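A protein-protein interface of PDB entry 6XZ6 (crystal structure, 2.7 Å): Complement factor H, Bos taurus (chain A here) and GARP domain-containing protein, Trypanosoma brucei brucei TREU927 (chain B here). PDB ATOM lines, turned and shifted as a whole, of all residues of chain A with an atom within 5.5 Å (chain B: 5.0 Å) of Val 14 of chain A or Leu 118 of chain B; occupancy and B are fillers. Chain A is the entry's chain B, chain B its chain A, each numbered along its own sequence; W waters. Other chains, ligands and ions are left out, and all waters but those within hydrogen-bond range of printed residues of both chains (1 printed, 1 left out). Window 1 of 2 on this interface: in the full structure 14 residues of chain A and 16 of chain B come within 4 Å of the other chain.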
ATOM      1  N   ILE A  10      -3.030 -33.991  35.397  1.00  0.00           N
ATOM      2  CA  ILE A  10      -4.073 -34.499  34.510  1.00  0.00           C
ATOM      3  C   ILE A  10      -3.444 -35.461  33.477  1.00  0.00           C
ATOM      4  O   ILE A  10      -3.193 -35.059  32.334  1.00  0.00           O
ATOM      5  CB  ILE A  10      -4.936 -33.370  33.842  1.00  0.00           C
ATOM      6  CG1 ILE A  10      -5.338 -32.290  34.864  1.00  0.00           C
ATOM      7  CG2 ILE A  10      -6.183 -33.959  33.164  1.00  0.00           C
ATOM      8  CD1 ILE A  10      -5.657 -30.998  34.321  1.00  0.00           C
ATOM      9  N   ASN A  12      -3.418 -38.027  30.455  1.00  0.00           N
ATOM     10  CA  ASN A  12      -4.258 -38.182  29.247  1.00  0.00           C
ATOM     11  C   ASN A  12      -5.124 -36.948  28.935  1.00  0.00           C
ATOM     12  O   ASN A  12      -6.118 -37.044  28.205  1.00  0.00           O
ATOM     13  CB  ASN A  12      -5.102 -39.468  29.295  1.00  0.00           C
ATOM     14  CG  ASN A  12      -4.273 -40.713  29.517  1.00  0.00           C
ATOM     15  OD1 ASN A  12      -3.368 -41.055  28.753  1.00  0.00           O
ATOM     16  ND2 ASN A  12      -4.559 -41.416  30.575  1.00  0.00           N
ATOM     17  N   GLY A  13      -4.676 -35.801  29.450  1.00  0.00           N
ATOM     18  CA  GLY A  13      -5.293 -34.497  29.260  1.00  0.00           C
ATOM     19  C   GLY A  13      -4.287 -33.367  29.196  1.00  0.00           C
ATOM     20  O   GLY A  13      -3.097 -33.586  29.451  1.00  0.00           O
ATOM     21  N   VAL A  14      -4.770 -32.149  28.851  1.00  0.00           N
ATOM     22  CA  VAL A  14      -3.986 -30.895  28.770  1.00  0.00           C
ATOM     23  C   VAL A  14      -4.740 -29.771  29.490  1.00  0.00           C
ATOM     24  O   VAL A  14      -5.895 -29.516  29.158  1.00  0.00           O
ATOM     25  CB  VAL A  14      -3.651 -30.374  27.336  1.00  0.00           C
ATOM     26  CG1 VAL A  14      -2.207 -29.951  27.169  1.00  0.00           C
ATOM     27  CG2 VAL A  14      -4.237 -31.170  26.188  1.00  0.00           C
ATOM     28  N   TYR A  15      -4.085 -29.065  30.411  1.00  0.00           N
ATOM     29  CA  TYR A  15      -4.662 -27.896  31.092  1.00  0.00           C
ATOM     30  C   TYR A  15      -3.955 -26.629  30.635  1.00  0.00           C
ATOM     31  O   TYR A  15      -2.876 -26.672  30.009  1.00  0.00           O
ATOM     32  CB  TYR A  15      -4.617 -28.013  32.628  1.00  0.00           C
ATOM     33  CG  TYR A  15      -3.228 -28.017  33.227  1.00  0.00           C
ATOM     34  CD1 TYR A  15      -2.504 -29.204  33.363  1.00  0.00           C
ATOM     35  CD2 TYR A  15      -2.650 -26.848  33.702  1.00  0.00           C
ATOM     36  CE1 TYR A  15      -1.215 -29.208  33.904  1.00  0.00           C
ATOM     37  CE2 TYR A  15      -1.365 -26.845  34.246  1.00  0.00           C
ATOM     38  CZ  TYR A  15      -0.655 -28.027  34.347  1.00  0.00           C
ATOM     39  OH  TYR A  15       0.600 -28.035  34.888  1.00  0.00           O
ATOM     40  N   ARG A  16      -4.589 -25.502  30.944  1.00  0.00           N
ATOM     41  CA  ARG A  16      -4.108 -24.161  30.681  1.00  0.00           C
ATOM     42  C   ARG A  16      -4.661 -23.216  31.775  1.00  0.00           C
ATOM     43  O   ARG A  16      -5.766 -23.464  32.270  1.00  0.00           O
ATOM     44  CB  ARG A  16      -4.451 -23.707  29.246  1.00  0.00           C
ATOM     45  CG  ARG A  16      -5.940 -23.558  28.897  1.00  0.00           C
ATOM     46  CD  ARG A  16      -6.287 -22.080  28.665  1.00  0.00           C
ATOM     47  NE  ARG A  16      -6.798 -21.462  29.895  1.00  0.00           N
ATOM     48  CZ  ARG A  16      -6.484 -20.248  30.323  1.00  0.00           C
ATOM     49  NH1 ARG A  16      -6.977 -19.797  31.475  1.00  0.00           N
ATOM     50  NH2 ARG A  16      -5.679 -19.471  29.602  1.00  0.00           N
ATOM     51  N   THR A  29      -8.468 -24.585  32.833  1.00  0.00           N
ATOM     52  CA  THR A  29      -9.395 -25.256  31.923  1.00  0.00           C
ATOM     53  C   THR A  29      -8.595 -26.428  31.307  1.00  0.00           C
ATOM     54  O   THR A  29      -7.427 -26.279  31.007  1.00  0.00           O
ATOM     55  CB  THR A  29     -10.014 -24.322  30.859  1.00  0.00           C
ATOM     56  OG1 THR A  29      -8.972 -23.728  30.098  1.00  0.00           O
ATOM     57  CG2 THR A  29     -10.934 -23.263  31.443  1.00  0.00           C
ATOM     58  N   TYR A  30      -9.196 -27.579  31.160  1.00  0.00           N
ATOM     59  CA  TYR A  30      -8.514 -28.743  30.614  1.00  0.00           C
ATOM     60  C   TYR A  30      -9.293 -29.427  29.480  1.00  0.00           C
ATOM     61  O   TYR A  30     -10.517 -29.362  29.435  1.00  0.00           O
ATOM     62  CB  TYR A  30      -8.171 -29.746  31.738  1.00  0.00           C
ATOM     63  CG  TYR A  30      -9.356 -30.510  32.294  1.00  0.00           C
ATOM     64  CD1 TYR A  30     -10.213 -29.927  33.229  1.00  0.00           C
ATOM     65  CD2 TYR A  30      -9.559 -31.851  31.973  1.00  0.00           C
ATOM     66  CE1 TYR A  30     -11.274 -30.639  33.774  1.00  0.00           C
ATOM     67  CE2 TYR A  30     -10.627 -32.569  32.507  1.00  0.00           C
ATOM     68  CZ  TYR A  30     -11.477 -31.961  33.409  1.00  0.00           C
ATOM     69  OH  TYR A  30     -12.534 -32.655  33.936  1.00  0.00           O
ATOM     70  N   GLU A  31      -8.564 -30.103  28.591  1.00  0.00           N
ATOM     71  CA  GLU A  31      -9.092 -30.873  27.465  1.00  0.00           C
ATOM     72  C   GLU A  31      -8.485 -32.260  27.539  1.00  0.00           C
ATOM     73  O   GLU A  31      -7.365 -32.407  28.000  1.00  0.00           O
ATOM     74  CB  GLU A  31      -8.727 -30.216  26.124  1.00  0.00           C
ATOM     75  CG  GLU A  31      -9.462 -28.924  25.856  1.00  0.00           C
ATOM     76  CD  GLU A  31     -10.957 -29.073  25.686  1.00  0.00           C
ATOM     77  OE1 GLU A  31     -11.371 -29.904  24.846  1.00  0.00           O
ATOM     78  OE2 GLU A  31     -11.712 -28.346  26.377  1.00  0.00           O
ATOM     79  N   CYS A  32      -9.215 -33.259  27.088  1.00  0.00           N
ATOM     80  CA  CYS A  32      -8.756 -34.638  27.094  1.00  0.00           C
ATOM     81  C   CYS A  32      -8.251 -35.062  25.696  1.00  0.00           C
ATOM     82  O   CYS A  32      -8.704 -34.530  24.677  1.00  0.00           O
ATOM     83  CB  CYS A  32      -9.855 -35.567  27.618  1.00  0.00           C
ATOM     84  SG  CYS A  32     -10.334 -35.282  29.356  1.00  0.00           S
ATOM     85  N   CYS A  58      -9.258 -37.310  33.165  1.00  0.00           N
ATOM     86  CA  CYS A  58      -9.516 -37.776  31.798  1.00  0.00           C
ATOM     87  C   CYS A  58      -9.572 -39.320  31.800  1.00  0.00           C
ATOM     88  O   CYS A  58      -8.575 -39.990  32.090  1.00  0.00           O
ATOM     89  CB  CYS A  58      -8.477 -37.239  30.817  1.00  0.00           C
ATOM     90  SG  CYS A  58      -8.618 -35.452  30.484  1.00  0.00           S
ATOM     91  N   LEU B  16      -0.715 -21.680  21.216  1.00  0.00           N
ATOM     92  CA  LEU B  16      -1.944 -22.464  20.980  1.00  0.00           C
ATOM     93  C   LEU B  16      -2.666 -21.959  19.729  1.00  0.00           C
ATOM     94  O   LEU B  16      -3.124 -22.742  18.915  1.00  0.00           O
ATOM     95  CB  LEU B  16      -2.905 -22.360  22.197  1.00  0.00           C
ATOM     96  CG  LEU B  16      -2.505 -23.056  23.518  1.00  0.00           C
ATOM     97  CD1 LEU B  16      -3.554 -22.841  24.552  1.00  0.00           C
ATOM     98  CD2 LEU B  16      -2.350 -24.548  23.333  1.00  0.00           C
ATOM     99  N   VAL B 114      -8.845 -30.251  20.316  1.00  0.00           N
ATOM    100  CA  VAL B 114      -8.121 -30.073  21.565  1.00  0.00           C
ATOM    101  C   VAL B 114      -7.622 -28.619  21.640  1.00  0.00           C
ATOM    102  O   VAL B 114      -7.977 -27.922  22.585  1.00  0.00           O
ATOM    103  CB  VAL B 114      -6.999 -31.151  21.771  1.00  0.00           C
ATOM    104  CG1 VAL B 114      -6.132 -30.845  23.003  1.00  0.00           C
ATOM    105  CG2 VAL B 114      -7.603 -32.555  21.869  1.00  0.00           C
ATOM    106  N   PHE B 115      -6.855 -28.156  20.635  1.00  0.00           N
ATOM    107  CA  PHE B 115      -6.333 -26.791  20.585  1.00  0.00           C
ATOM    108  C   PHE B 115      -7.436 -25.747  20.546  1.00  0.00           C
ATOM    109  O   PHE B 115      -7.264 -24.685  21.132  1.00  0.00           O
ATOM    110  CB  PHE B 115      -5.385 -26.615  19.414  1.00  0.00           C
ATOM    111  CG  PHE B 115      -4.063 -27.276  19.668  1.00  0.00           C
ATOM    112  CD1 PHE B 115      -3.034 -26.585  20.297  1.00  0.00           C
ATOM    113  CD2 PHE B 115      -3.834 -28.587  19.264  1.00  0.00           C
ATOM    114  CE1 PHE B 115      -1.802 -27.196  20.523  1.00  0.00           C
ATOM    115  CE2 PHE B 115      -2.608 -29.204  19.503  1.00  0.00           C
ATOM    116  CZ  PHE B 115      -1.599 -28.507  20.131  1.00  0.00           C
ATOM    117  N   SER B 116      -8.557 -26.039  19.876  1.00  0.00           N
ATOM    118  CA  SER B 116      -9.723 -25.157  19.827  1.00  0.00           C
ATOM    119  C   SER B 116     -10.395 -25.027  21.211  1.00  0.00           C
ATOM    120  O   SER B 116     -10.750 -23.930  21.597  1.00  0.00           O
ATOM    121  CB  SER B 116     -10.718 -25.633  18.763  1.00  0.00           C
ATOM    122  OG  SER B 116     -10.192 -25.399  17.466  1.00  0.00           O
ATOM    123  N   GLY B 117     -10.505 -26.129  21.946  1.00  0.00           N
ATOM    124  CA  GLY B 117     -11.059 -26.176  23.296  1.00  0.00           C
ATOM    125  C   GLY B 117     -10.185 -25.481  24.316  1.00  0.00           C
ATOM    126  O   GLY B 117     -10.701 -24.803  25.205  1.00  0.00           O
ATOM    127  N   LEU B 118      -8.862 -25.609  24.188  1.00  0.00           N
ATOM    128  CA  LEU B 118      -7.935 -24.919  25.075  1.00  0.00           C
ATOM    129  C   LEU B 118      -8.071 -23.416  24.878  1.00  0.00           C
ATOM    130  O   LEU B 118      -8.105 -22.675  25.865  1.00  0.00           O
ATOM    131  CB  LEU B 118      -6.473 -25.374  24.877  1.00  0.00           C
ATOM    132  CG  LEU B 118      -6.129 -26.797  25.396  1.00  0.00           C
ATOM    133  CD1 LEU B 118      -4.789 -27.273  24.874  1.00  0.00           C
ATOM    134  CD2 LEU B 118      -6.171 -26.882  26.903  1.00  0.00           C
ATOM    135  N   LEU B 119      -8.251 -22.971  23.628  1.00  0.00           N
ATOM    136  CA  LEU B 119      -8.414 -21.552  23.327  1.00  0.00           C
ATOM    137  C   LEU B 119      -9.728 -21.029  23.844  1.00  0.00           C
ATOM    138  O   LEU B 119      -9.760 -19.928  24.381  1.00  0.00           O
ATOM    139  CB  LEU B 119      -8.268 -21.271  21.830  1.00  0.00           C
ATOM    140  CG  LEU B 119      -6.859 -21.348  21.281  1.00  0.00           C
ATOM    141  CD1 LEU B 119      -6.906 -21.612  19.792  1.00  0.00           C
ATOM    142  CD2 LEU B 119      -6.072 -20.055  21.603  1.00  0.00           C
ATOM    143  N   ARG B 120     -10.801 -21.822  23.724  1.00  0.00           N
ATOM    144  CA  ARG B 120     -12.134 -21.485  24.207  1.00  0.00           C
ATOM    145  C   ARG B 120     -12.068 -21.212  25.715  1.00  0.00           C
ATOM    146  O   ARG B 120     -12.680 -20.252  26.173  1.00  0.00           O
ATOM    147  CB  ARG B 120     -13.084 -22.624  23.913  1.00  0.00           C
ATOM    148  CG  ARG B 120     -14.296 -22.221  23.114  1.00  0.00           C
ATOM    149  CD  ARG B 120     -15.265 -23.406  22.988  1.00  0.00           C
ATOM    150  NE  ARG B 120     -14.824 -24.336  21.951  1.00  0.00           N
ATOM    151  CZ  ARG B 120     -14.479 -25.592  22.169  1.00  0.00           C
ATOM    152  NH1 ARG B 120     -14.554 -26.106  23.391  1.00  0.00           N
ATOM    153  NH2 ARG B 120     -14.075 -26.353  21.169  1.00  0.00           N
ATOM    154  N   GLY B 121     -11.299 -22.029  26.458  1.00  0.00           N
ATOM    155  CA  GLY B 121     -11.035 -21.869  27.886  1.00  0.00           C
ATOM    156  C   GLY B 121     -10.352 -20.549  28.181  1.00  0.00           C
ATOM    157  O   GLY B 121     -10.803 -19.821  29.063  1.00  0.00           O
ATOM    158  N   ALA B 122      -9.286 -20.203  27.409  1.00  0.00           N
ATOM    159  CA  ALA B 122      -8.550 -18.914  27.492  1.00  0.00           C
ATOM    160  C   ALA B 122      -9.479 -17.713  27.127  1.00  0.00           C
ATOM    161  O   ALA B 122      -9.348 -16.633  27.722  1.00  0.00           O
ATOM    162  CB  ALA B 122      -7.322 -18.936  26.589  1.00  0.00           C
ATOM    163  N   GLN B 164       4.003 -30.060  29.939  1.00  0.00           N
ATOM    164  CA  GLN B 164       3.069 -31.173  29.873  1.00  0.00           C
ATOM    165  C   GLN B 164       3.454 -32.112  28.762  1.00  0.00           C
ATOM    166  O   GLN B 164       3.910 -31.655  27.711  1.00  0.00           O
ATOM    167  CB  GLN B 164       1.648 -30.669  29.646  1.00  0.00           C
ATOM    168  CG  GLN B 164       1.007 -30.101  30.882  1.00  0.00           C
ATOM    169  CD  GLN B 164      -0.330 -29.560  30.530  1.00  0.00           C
ATOM    170  OE1 GLN B 164      -1.327 -30.280  30.630  1.00  0.00           O
ATOM    171  NE2 GLN B 164      -0.377 -28.286  30.098  1.00  0.00           N
ATOM    172  N   PHE B 166       1.660 -33.767  26.750  1.00  0.00           N
ATOM    173  CA  PHE B 166       0.858 -33.513  25.558  1.00  0.00           C
ATOM    174  C   PHE B 166       1.583 -32.697  24.491  1.00  0.00           C
ATOM    175  O   PHE B 166       1.497 -33.017  23.307  1.00  0.00           O
ATOM    176  CB  PHE B 166      -0.465 -32.837  25.940  1.00  0.00           C
ATOM    177  CG  PHE B 166      -1.294 -32.428  24.743  1.00  0.00           C
ATOM    178  CD1 PHE B 166      -1.244 -31.127  24.252  1.00  0.00           C
ATOM    179  CD2 PHE B 166      -2.098 -33.356  24.084  1.00  0.00           C
ATOM    180  CE1 PHE B 166      -2.005 -30.749  23.143  1.00  0.00           C
ATOM    181  CE2 PHE B 166      -2.852 -32.978  22.971  1.00  0.00           C
ATOM    182  CZ  PHE B 166      -2.790 -31.677  22.502  1.00  0.00           C
HETATM  183  O   HOH W   1      -0.046 -33.994  29.297  1.00  0.00           O
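O of Tyr 15 of chain A lies within hydrogen-bond range of NE2 of Gln 164 of chain B (3.0 Å).
Val 14 of chain A touches just these residues of chain B: Val 114 (3.7 Å), Leu 118 (3.5 Å), Gln 164 (3.3 Å) and Phe 166 (3.3 Å).
Leu 118 of chain B touches just these residues of chain A: Val 14 (3.5 Å), Arg 16 (3.4 Å) and Glu 31 (3.8 Å).
Printed residues of chain B within 4 Å of Gly 13 of chain A: Gln 164.
Printed residues of chain A within 4 Å of Gln 164 of chain B: Gly 13, Val 14 and Tyr 15.
Ser 116 of chain B touches none of the printed residues of chain A.
Phe 115 of chain B touches none of the printed residues of chain A.
The nearest printed residue of chain B that does not touch Val 14 of chain A is Leu 16 of chain B (6.6 Å).
Water W1 bridges the backbone NH of Phe 166 of chain B (3.1 Å) and the backbone carbonyl oxygen of Gly 13 of chain A (3.1 Å).
O of Gly 13 of chain A touches OE1 of Gln 164 of chain B (3.9 Å).
Val 114 of chain B touches Val 14 of chain A (CG1 to CG2, 3.7 Å).
Val 14 of chain A touches Leu 118 of chain B.
CA of Val 14 of chain A touches OE1 of Gln 164 of chain B, at 3.3 Å.
Phe 166 of chain B touches Val 14 of chain A (CD1 to CG1, 3.3 Å).
O of Leu 118 of chain B touches CD of Arg 16 of chain A, at 3.4 Å.
Arg 16 of chain A touches Ala 122 of chain B.
Thr 29 of chain A touches Gly 121 of chain B (OG1 to CA, 3.6 Å).
Glu 31 of chain A touches Val 114 of chain B (CG to O, 3.7 Å).
Glu 31 of chain A touches Leu 118 of chain B (CG to N, 3.8 Å).
Of the 12 printed residues of chain B, 7 touch a printed residue of chain A.
Printed residues of chain B that touch a printed residue of chain A: Val 114, Gly 117, Leu 118, Gly 121, Ala 122, Gln 164 and Phe 166.
Of the 11 printed residues of chain A, 7 touch a printed residue of chain B.
Printed residues of chain A that touch a printed residue of chain B: Gly 13, Val 14, Tyr 15, Arg 16, Thr 29, Glu 31 and Cys 32.
Among the printed residues, no Asp or Glu carboxylate lies within 4 Å of a Lys or Arg side-chain nitrogen of the other chain.
N of Arg 16 of chain A is in hydrogen-bond range of O of Thr 29 of chain A (2.9 Å).
The side-chain sulfur of Cys 32 of chain A forms a disulfide with the side-chain sulfur of Cys 58 of chain A.
The backbone NH (N) of Val 14 of chain A lies within hydrogen-bond range of the backbone carbonyl oxygen (O) of Glu 31 of chain A (2.7 Å).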
